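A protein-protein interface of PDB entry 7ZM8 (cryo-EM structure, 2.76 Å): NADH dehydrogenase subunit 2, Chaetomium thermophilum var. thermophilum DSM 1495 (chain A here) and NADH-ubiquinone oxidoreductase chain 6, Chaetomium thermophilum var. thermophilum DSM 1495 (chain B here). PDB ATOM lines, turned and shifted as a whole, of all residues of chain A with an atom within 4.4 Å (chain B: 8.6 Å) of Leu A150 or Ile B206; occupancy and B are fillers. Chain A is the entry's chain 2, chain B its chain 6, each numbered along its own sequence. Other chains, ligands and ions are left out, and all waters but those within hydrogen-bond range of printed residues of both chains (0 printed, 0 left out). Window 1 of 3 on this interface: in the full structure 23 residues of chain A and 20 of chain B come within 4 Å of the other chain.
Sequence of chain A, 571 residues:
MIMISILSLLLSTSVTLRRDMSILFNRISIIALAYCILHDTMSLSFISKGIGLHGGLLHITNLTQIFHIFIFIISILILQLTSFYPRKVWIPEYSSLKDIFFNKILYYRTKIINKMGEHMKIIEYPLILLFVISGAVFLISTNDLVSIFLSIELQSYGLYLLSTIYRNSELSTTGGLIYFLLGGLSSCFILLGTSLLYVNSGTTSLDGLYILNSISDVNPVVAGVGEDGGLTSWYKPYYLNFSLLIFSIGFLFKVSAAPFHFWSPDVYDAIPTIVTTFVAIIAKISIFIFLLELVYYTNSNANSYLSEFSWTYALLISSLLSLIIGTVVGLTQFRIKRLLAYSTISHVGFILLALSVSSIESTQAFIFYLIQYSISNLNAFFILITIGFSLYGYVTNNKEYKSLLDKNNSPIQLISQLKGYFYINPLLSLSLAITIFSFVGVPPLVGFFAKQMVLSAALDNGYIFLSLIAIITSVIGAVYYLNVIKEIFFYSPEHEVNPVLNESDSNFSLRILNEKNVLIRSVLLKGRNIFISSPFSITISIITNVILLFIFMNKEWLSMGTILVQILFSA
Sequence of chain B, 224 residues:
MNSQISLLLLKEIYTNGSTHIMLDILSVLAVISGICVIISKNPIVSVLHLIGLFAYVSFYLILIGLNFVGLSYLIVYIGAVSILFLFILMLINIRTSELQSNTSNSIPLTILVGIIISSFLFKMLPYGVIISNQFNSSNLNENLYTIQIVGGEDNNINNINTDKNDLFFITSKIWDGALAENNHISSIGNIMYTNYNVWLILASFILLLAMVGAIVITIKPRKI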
ATOM      1  N   VAL A 146     -15.309  -8.857  -4.807  1.00  0.00           N
ATOM      2  CA  VAL A 146     -15.238  -8.258  -6.133  1.00  0.00           C
ATOM      3  C   VAL A 146     -16.011  -6.949  -6.163  1.00  0.00           C
ATOM      4  O   VAL A 146     -15.552  -5.951  -6.726  1.00  0.00           O
ATOM      5  CB  VAL A 146     -15.780  -9.251  -7.173  1.00  0.00           C
ATOM      6  CG1 VAL A 146     -15.510  -8.780  -8.599  1.00  0.00           C
ATOM      7  CG2 VAL A 146     -15.271 -10.653  -6.892  1.00  0.00           C
ATOM      8  N   SER A 147     -17.194  -6.948  -5.557  1.00  0.00           N
ATOM      9  CA  SER A 147     -18.046  -5.738  -5.580  1.00  0.00           C
ATOM     10  C   SER A 147     -17.341  -4.609  -4.828  1.00  0.00           C
ATOM     11  O   SER A 147     -17.428  -3.475  -5.301  1.00  0.00           O
ATOM     12  CB  SER A 147     -19.397  -6.058  -5.006  1.00  0.00           C
ATOM     13  OG  SER A 147     -20.042  -7.074  -5.753  1.00  0.00           O
ATOM     14  N   ILE A 148     -16.620  -4.915  -3.748  1.00  0.00           N
ATOM     15  CA  ILE A 148     -15.847  -3.901  -3.038  1.00  0.00           C
ATOM     16  C   ILE A 148     -14.838  -3.262  -3.974  1.00  0.00           C
ATOM     17  O   ILE A 148     -14.763  -2.035  -4.093  1.00  0.00           O
ATOM     18  CB  ILE A 148     -15.147  -4.524  -1.818  1.00  0.00           C
ATOM     19  CG1 ILE A 148     -16.158  -4.861  -0.732  1.00  0.00           C
ATOM     20  CG2 ILE A 148     -14.081  -3.591  -1.281  1.00  0.00           C
ATOM     21  CD1 ILE A 148     -15.615  -5.790   0.300  1.00  0.00           C
ATOM     22  N   PHE A 149     -14.056  -4.090  -4.665  1.00  0.00           N
ATOM     23  CA  PHE A 149     -13.002  -3.566  -5.519  1.00  0.00           C
ATOM     24  C   PHE A 149     -13.573  -2.728  -6.651  1.00  0.00           C
ATOM     25  O   PHE A 149     -13.059  -1.646  -6.952  1.00  0.00           O
ATOM     26  CB  PHE A 149     -12.164  -4.710  -6.080  1.00  0.00           C
ATOM     27  CG  PHE A 149     -11.138  -4.262  -7.068  1.00  0.00           C
ATOM     28  CD1 PHE A 149     -10.026  -3.557  -6.650  1.00  0.00           C
ATOM     29  CD2 PHE A 149     -11.297  -4.517  -8.412  1.00  0.00           C
ATOM     30  CE1 PHE A 149      -9.096  -3.128  -7.555  1.00  0.00           C
ATOM     31  CE2 PHE A 149     -10.368  -4.091  -9.316  1.00  0.00           C
ATOM     32  CZ  PHE A 149      -9.265  -3.399  -8.888  1.00  0.00           C
ATOM     33  N   LEU A 150     -14.638  -3.210  -7.287  1.00  0.00           N
ATOM     34  CA  LEU A 150     -15.226  -2.485  -8.402  1.00  0.00           C
ATOM     35  C   LEU A 150     -15.859  -1.180  -7.941  1.00  0.00           C
ATOM     36  O   LEU A 150     -15.829  -0.181  -8.666  1.00  0.00           O
ATOM     37  CB  LEU A 150     -16.258  -3.363  -9.104  1.00  0.00           C
ATOM     38  CG  LEU A 150     -15.746  -4.358 -10.149  1.00  0.00           C
ATOM     39  CD1 LEU A 150     -16.700  -5.515 -10.282  1.00  0.00           C
ATOM     40  CD2 LEU A 150     -15.562  -3.687 -11.486  1.00  0.00           C
ATOM     41  N   SER A 151     -16.441  -1.168  -6.741  1.00  0.00           N
ATOM     42  CA  SER A 151     -17.060   0.049  -6.231  1.00  0.00           C
ATOM     43  C   SER A 151     -16.018   1.077  -5.817  1.00  0.00           C
ATOM     44  O   SER A 151     -16.179   2.270  -6.091  1.00  0.00           O
ATOM     45  CB  SER A 151     -17.971  -0.276  -5.052  1.00  0.00           C
ATOM     46  OG  SER A 151     -18.938  -1.232  -5.417  1.00  0.00           O
ATOM     47  N   ILE A 152     -14.940   0.632  -5.179  1.00  0.00           N
ATOM     48  CA  ILE A 152     -13.926   1.594  -4.667  1.00  0.00           C
ATOM     49  C   ILE A 152     -13.287   2.298  -5.855  1.00  0.00           C
ATOM     50  O   ILE A 152     -13.100   3.513  -5.767  1.00  0.00           O
ATOM     51  CB  ILE A 152     -12.919   0.971  -3.663  1.00  0.00           C
ATOM     52  CG1 ILE A 152     -12.171   2.048  -2.876  1.00  0.00           C
ATOM     53  CG2 ILE A 152     -11.961  -0.007  -4.321  1.00  0.00           C
ATOM     54  CD1 ILE A 152     -13.074   3.034  -2.177  1.00  0.00           C
ATOM     55  N   GLU A 153     -12.985   1.558  -6.917  1.00  0.00           N
ATOM     56  CA  GLU A 153     -12.423   2.148  -8.158  1.00  0.00           C
ATOM     57  C   GLU A 153     -13.429   3.089  -8.825  1.00  0.00           C
ATOM     58  O   GLU A 153     -13.018   4.168  -9.223  1.00  0.00           O
ATOM     59  CB  GLU A 153     -11.953   1.040  -9.101  1.00  0.00           C
ATOM     60  CG  GLU A 153     -10.917   0.123  -8.477  1.00  0.00           C
ATOM     61  CD  GLU A 153      -9.653   0.791  -7.960  1.00  0.00           C
ATOM     62  OE1 GLU A 153      -8.744   1.039  -8.773  1.00  0.00           O
ATOM     63  OE2 GLU A 153      -9.576   1.053  -6.744  1.00  0.00           O
ATOM     64  N   LEU A 154     -14.702   2.711  -8.900  1.00  0.00           N
ATOM     65  CA  LEU A 154     -15.727   3.634  -9.442  1.00  0.00           C
ATOM     66  C   LEU A 154     -15.674   4.969  -8.688  1.00  0.00           C
ATOM     67  O   LEU A 154     -15.776   6.012  -9.347  1.00  0.00           O
ATOM     68  CB  LEU A 154     -17.113   2.999  -9.340  1.00  0.00           C
ATOM     69  CG  LEU A 154     -18.232   3.692 -10.112  1.00  0.00           C
ATOM     70  CD1 LEU A 154     -17.769   4.116 -11.497  1.00  0.00           C
ATOM     71  CD2 LEU A 154     -19.442   2.782 -10.215  1.00  0.00           C
ATOM     72  N   TYR B 196     -23.962 -13.431 -11.602  1.00  0.00           N
ATOM     73  CA  TYR B 196     -23.037 -12.370 -11.122  1.00  0.00           C
ATOM     74  C   TYR B 196     -23.169 -11.152 -12.038  1.00  0.00           C
ATOM     75  O   TYR B 196     -22.160 -10.459 -12.233  1.00  0.00           O
ATOM     76  CB  TYR B 196     -21.614 -12.916 -11.007  1.00  0.00           C
ATOM     77  CG  TYR B 196     -21.461 -14.108 -10.097  1.00  0.00           C
ATOM     78  CD1 TYR B 196     -21.529 -15.400 -10.591  1.00  0.00           C
ATOM     79  CD2 TYR B 196     -21.257 -13.945  -8.740  1.00  0.00           C
ATOM     80  CE1 TYR B 196     -21.397 -16.498  -9.760  1.00  0.00           C
ATOM     81  CE2 TYR B 196     -21.121 -15.032  -7.894  1.00  0.00           C
ATOM     82  CZ  TYR B 196     -21.192 -16.314  -8.406  1.00  0.00           C
ATOM     83  OH  TYR B 196     -21.057 -17.388  -7.577  1.00  0.00           O
ATOM     84  N   ASN B 197     -24.370 -10.886 -12.559  1.00  0.00           N
ATOM     85  CA  ASN B 197     -24.595  -9.784 -13.538  1.00  0.00           C
ATOM     86  C   ASN B 197     -24.329  -8.395 -12.943  1.00  0.00           C
ATOM     87  O   ASN B 197     -24.136  -7.463 -13.729  1.00  0.00           O
ATOM     88  CB  ASN B 197     -25.931  -9.932 -14.281  1.00  0.00           C
ATOM     89  CG  ASN B 197     -27.163  -9.807 -13.414  1.00  0.00           C
ATOM     90  OD1 ASN B 197     -27.072  -9.589 -12.209  1.00  0.00           O
ATOM     91  ND2 ASN B 197     -28.327  -9.944 -14.024  1.00  0.00           N
ATOM     92  N   VAL B 198     -24.382  -8.251 -11.621  1.00  0.00           N
ATOM     93  CA  VAL B 198     -24.124  -6.942 -10.941  1.00  0.00           C
ATOM     94  C   VAL B 198     -22.684  -6.492 -11.219  1.00  0.00           C
ATOM     95  O   VAL B 198     -22.473  -5.282 -11.384  1.00  0.00           O
ATOM     96  CB  VAL B 198     -24.488  -6.991  -9.441  1.00  0.00           C
ATOM     97  CG1 VAL B 198     -23.518  -6.226  -8.552  1.00  0.00           C
ATOM     98  CG2 VAL B 198     -25.915  -6.531  -9.204  1.00  0.00           C
ATOM     99  N   TRP B 199     -21.738  -7.428 -11.277  1.00  0.00           N
ATOM    100  CA  TRP B 199     -20.327  -7.084 -11.612  1.00  0.00           C
ATOM    101  C   TRP B 199     -20.244  -6.498 -13.024  1.00  0.00           C
ATOM    102  O   TRP B 199     -19.467  -5.559 -13.209  1.00  0.00           O
ATOM    103  CB  TRP B 199     -19.408  -8.296 -11.461  1.00  0.00           C
ATOM    104  CG  TRP B 199     -19.332  -8.869 -10.082  1.00  0.00           C
ATOM    105  CD1 TRP B 199     -19.689  -8.268  -8.912  1.00  0.00           C
ATOM    106  CD2 TRP B 199     -18.845 -10.175  -9.730  1.00  0.00           C
ATOM    107  NE1 TRP B 199     -19.466  -9.113  -7.859  1.00  0.00           N
ATOM    108  CE2 TRP B 199     -18.951 -10.290  -8.329  1.00  0.00           C
ATOM    109  CE3 TRP B 199     -18.332 -11.252 -10.460  1.00  0.00           C
ATOM    110  CZ2 TRP B 199     -18.568 -11.442  -7.648  1.00  0.00           C
ATOM    111  CZ3 TRP B 199     -17.950 -12.388  -9.786  1.00  0.00           C
ATOM    112  CH2 TRP B 199     -18.063 -12.477  -8.399  1.00  0.00           C
ATOM    113  N   LEU B 200     -21.000  -7.045 -13.976  1.00  0.00           N
ATOM    114  CA  LEU B 200     -21.022  -6.528 -15.366  1.00  0.00           C
ATOM    115  C   LEU B 200     -21.580  -5.107 -15.361  1.00  0.00           C
ATOM    116  O   LEU B 200     -21.030  -4.260 -16.063  1.00  0.00           O
ATOM    117  CB  LEU B 200     -21.920  -7.453 -16.192  1.00  0.00           C
ATOM    118  CG  LEU B 200     -21.896  -7.250 -17.705  1.00  0.00           C
ATOM    119  CD1 LEU B 200     -20.536  -7.606 -18.281  1.00  0.00           C
ATOM    120  CD2 LEU B 200     -22.984  -8.081 -18.360  1.00  0.00           C
ATOM    121  N   ILE B 201     -22.638  -4.877 -14.593  1.00  0.00           N
ATOM    122  CA  ILE B 201     -23.274  -3.532 -14.515  1.00  0.00           C
ATOM    123  C   ILE B 201     -22.287  -2.515 -13.929  1.00  0.00           C
ATOM    124  O   ILE B 201     -22.228  -1.394 -14.439  1.00  0.00           O
ATOM    125  CB  ILE B 201     -24.594  -3.606 -13.719  1.00  0.00           C
ATOM    126  CG1 ILE B 201     -25.623  -4.494 -14.423  1.00  0.00           C
ATOM    127  CG2 ILE B 201     -25.151  -2.219 -13.441  1.00  0.00           C
ATOM    128  CD1 ILE B 201     -25.806  -4.176 -15.890  1.00  0.00           C
ATOM    129  N   LEU B 202     -21.500  -2.908 -12.932  1.00  0.00           N
ATOM    130  CA  LEU B 202     -20.620  -1.927 -12.263  1.00  0.00           C
ATOM    131  C   LEU B 202     -19.397  -1.680 -13.132  1.00  0.00           C
ATOM    132  O   LEU B 202     -18.880  -0.552 -13.108  1.00  0.00           O
ATOM    133  CB  LEU B 202     -20.167  -2.539 -10.936  1.00  0.00           C
ATOM    134  CG  LEU B 202     -21.015  -2.199  -9.713  1.00  0.00           C
ATOM    135  CD1 LEU B 202     -20.470  -2.899  -8.475  1.00  0.00           C
ATOM    136  CD2 LEU B 202     -21.055  -0.698  -9.494  1.00  0.00           C
ATOM    137  N   ALA B 203     -18.969  -2.703 -13.873  1.00  0.00           N
ATOM    138  CA  ALA B 203     -17.846  -2.531 -14.783  1.00  0.00           C
ATOM    139  C   ALA B 203     -18.239  -1.717 -16.005  1.00  0.00           C
ATOM    140  O   ALA B 203     -17.433  -0.934 -16.520  1.00  0.00           O
ATOM    141  CB  ALA B 203     -17.307  -3.895 -15.197  1.00  0.00           C
ATOM    142  N   SER B 204     -19.464  -1.895 -16.493  1.00  0.00           N
ATOM    143  CA  SER B 204     -19.935  -1.085 -17.610  1.00  0.00           C
ATOM    144  C   SER B 204     -19.959   0.391 -17.242  1.00  0.00           C
ATOM    145  O   SER B 204     -19.699   1.255 -18.086  1.00  0.00           O
ATOM    146  CB  SER B 204     -21.321  -1.554 -18.048  1.00  0.00           C
ATOM    147  OG  SER B 204     -22.282  -1.287 -17.046  1.00  0.00           O
ATOM    148  N   PHE B 205     -20.280   0.699 -15.989  1.00  0.00           N
ATOM    149  CA  PHE B 205     -20.262   2.081 -15.541  1.00  0.00           C
ATOM    150  C   PHE B 205     -18.847   2.586 -15.295  1.00  0.00           C
ATOM    151  O   PHE B 205     -18.602   3.790 -15.405  1.00  0.00           O
ATOM    152  CB  PHE B 205     -21.125   2.227 -14.288  1.00  0.00           C
ATOM    153  CG  PHE B 205     -22.570   2.499 -14.586  1.00  0.00           C
ATOM    154  CD1 PHE B 205     -23.020   3.791 -14.787  1.00  0.00           C
ATOM    155  CD2 PHE B 205     -23.478   1.463 -14.680  1.00  0.00           C
ATOM    156  CE1 PHE B 205     -24.346   4.042 -15.062  1.00  0.00           C
ATOM    157  CE2 PHE B 205     -24.807   1.709 -14.961  1.00  0.00           C
ATOM    158  CZ  PHE B 205     -25.240   2.998 -15.151  1.00  0.00           C
ATOM    159  N   ILE B 206     -17.908   1.695 -14.967  1.00  0.00           N
ATOM    160  CA  ILE B 206     -16.509   2.097 -14.839  1.00  0.00           C
ATOM    161  C   ILE B 206     -15.929   2.441 -16.202  1.00  0.00           C
ATOM    162  O   ILE B 206     -15.210   3.433 -16.349  1.00  0.00           O
ATOM    163  CB  ILE B 206     -15.694   0.992 -14.141  1.00  0.00           C
ATOM    164  CG1 ILE B 206     -15.907   1.040 -12.632  1.00  0.00           C
ATOM    165  CG2 ILE B 206     -14.218   1.122 -14.449  1.00  0.00           C
ATOM    166  CD1 ILE B 206     -15.201  -0.058 -11.893  1.00  0.00           C
ATOM    167  N   LEU B 207     -16.224   1.625 -17.216  1.00  0.00           N
ATOM    168  CA  LEU B 207     -15.802   1.938 -18.577  1.00  0.00           C
ATOM    169  C   LEU B 207     -16.480   3.201 -19.085  1.00  0.00           C
ATOM    170  O   LEU B 207     -15.865   4.006 -19.791  1.00  0.00           O
ATOM    171  CB  LEU B 207     -16.115   0.763 -19.501  1.00  0.00           C
ATOM    172  CG  LEU B 207     -15.347  -0.536 -19.273  1.00  0.00           C
ATOM    173  CD1 LEU B 207     -16.165  -1.718 -19.759  1.00  0.00           C
ATOM    174  CD2 LEU B 207     -14.011  -0.487 -19.975  1.00  0.00           C
ATOM    175  N   LEU B 208     -17.757   3.377 -18.751  1.00  0.00           N
ATOM    176  CA  LEU B 208     -18.484   4.583 -19.121  1.00  0.00           C
ATOM    177  C   LEU B 208     -17.844   5.826 -18.517  1.00  0.00           C
ATOM    178  O   LEU B 208     -17.788   6.879 -19.158  1.00  0.00           O
ATOM    179  CB  LEU B 208     -19.939   4.450 -18.673  1.00  0.00           C
ATOM    180  CG  LEU B 208     -20.971   5.469 -19.131  1.00  0.00           C
ATOM    181  CD1 LEU B 208     -21.129   5.410 -20.622  1.00  0.00           C
ATOM    182  CD2 LEU B 208     -22.281   5.185 -18.458  1.00  0.00           C
ATOM    183  N   LEU B 209     -17.368   5.726 -17.274  1.00  0.00           N
ATOM    184  CA  LEU B 209     -16.686   6.847 -16.639  1.00  0.00           C
ATOM    185  C   LEU B 209     -15.336   7.122 -17.292  1.00  0.00           C
ATOM    186  O   LEU B 209     -14.955   8.282 -17.476  1.00  0.00           O
ATOM    187  CB  LEU B 209     -16.517   6.571 -15.149  1.00  0.00           C
ATOM    188  CG  LEU B 209     -15.785   7.618 -14.315  1.00  0.00           C
ATOM    189  CD1 LEU B 209     -16.625   8.861 -14.179  1.00  0.00           C
ATOM    190  CD2 LEU B 209     -15.439   7.057 -12.954  1.00  0.00           C
ATOM    191  N   ALA B 210     -14.595   6.071 -17.635  1.00  0.00           N
ATOM    192  CA  ALA B 210     -13.305   6.260 -18.281  1.00  0.00           C
ATOM    193  C   ALA B 210     -13.454   6.842 -19.678  1.00  0.00           C
ATOM    194  O   ALA B 210     -12.497   7.406 -20.218  1.00  0.00           O
ATOM    195  CB  ALA B 210     -12.546   4.937 -18.330  1.00  0.00           C
ATOM    196  N   MET B 211     -14.633   6.708 -20.282  1.00  0.00           N
ATOM    197  CA  MET B 211     -14.882   7.311 -21.583  1.00  0.00           C
ATOM    198  C   MET B 211     -15.186   8.795 -21.453  1.00  0.00           C
ATOM    199  O   MET B 211     -14.508   9.630 -22.057  1.00  0.00           O
ATOM    200  CB  MET B 211     -16.038   6.596 -22.275  1.00  0.00           C
ATOM    201  CG  MET B 211     -16.502   7.262 -23.554  1.00  0.00           C
ATOM    202  SD  MET B 211     -15.393   6.944 -24.932  1.00  0.00           S
ATOM    203  CE  MET B 211     -15.857   5.266 -25.336  1.00  0.00           C
ATOM    204  N   VAL B 212     -16.206   9.131 -20.669  1.00  0.00           N
ATOM    205  CA  VAL B 212     -16.614  10.520 -20.515  1.00  0.00           C
ATOM    206  C   VAL B 212     -15.517  11.335 -19.846  1.00  0.00           C
ATOM    207  O   VAL B 212     -15.205  12.451 -20.274  1.00  0.00           O
ATOM    208  CB  VAL B 212     -17.931  10.584 -19.723  1.00  0.00           C
ATOM    209  CG1 VAL B 212     -18.241  12.008 -19.306  1.00  0.00           C
ATOM    210  CG2 VAL B 212     -19.056   9.999 -20.542  1.00  0.00           C
ATOM    211  N   GLY B 213     -14.914  10.791 -18.788  1.00  0.00           N
ATOM    212  CA  GLY B 213     -13.948  11.558 -18.025  1.00  0.00           C
ATOM    213  C   GLY B 213     -12.665  11.839 -18.781  1.00  0.00           C
ATOM    214  O   GLY B 213     -12.095  12.924 -18.665  1.00  0.00           O
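OG of Ser A147 is in hydrogen-bond range of NE1 of Trp B199 (3.0 Å).
OG of Ser A151 lies within hydrogen-bond range of O of Ser A147, 2.7 Å away.
CG2 of Val A146 touches CZ2 of Trp B199, at 3.5 Å.
O of Leu A150 touches CD1 of Ile B206, at 3.3 Å.
Ser A151 touches Leu B202 (OG to CD1, 3.8 Å).
Leu A154 touches Leu B202.
Leu A154 touches Ile B206 (CD1 to CG1, 3.8 Å).
Leu B209 touches Leu A154 (CD2 to O, 3.8 Å).
Of chain B, only Ile B206 (3.3 Å) comes within 4 Å of Leu A150.
Ile B206 touches just these residues of chain A: Leu A150 (3.3 Å) and Leu A154 (3.8 Å).
Of the printed residues of chain A, Leu B209 touches Leu A154.
Of the printed residues of chain A, Leu B202 touches Ser A151 and Leu A154.
Glu A153 touches none of the printed residues of chain B.
Ala B203 touches none of the printed residues of chain A.
The nearest printed residue of chain A that does not touch Ile B206 is Glu A153 (4.4 Å).
The nearest printed residue of chain B that does not touch Val A146 is Leu B202 (6.0 Å).
Of the 9 printed residues of chain A, 5 touch a printed residue of chain B.
Printed residues of chain A that touch a printed residue of chain B: Val A146, Ser A147, Leu A150, Ser A151 and Leu A154.
Hydrophobic or aromatic side chains of chain B that line the printed part of chain A: Trp B199, Leu B202, Ile B206 and Leu B209.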
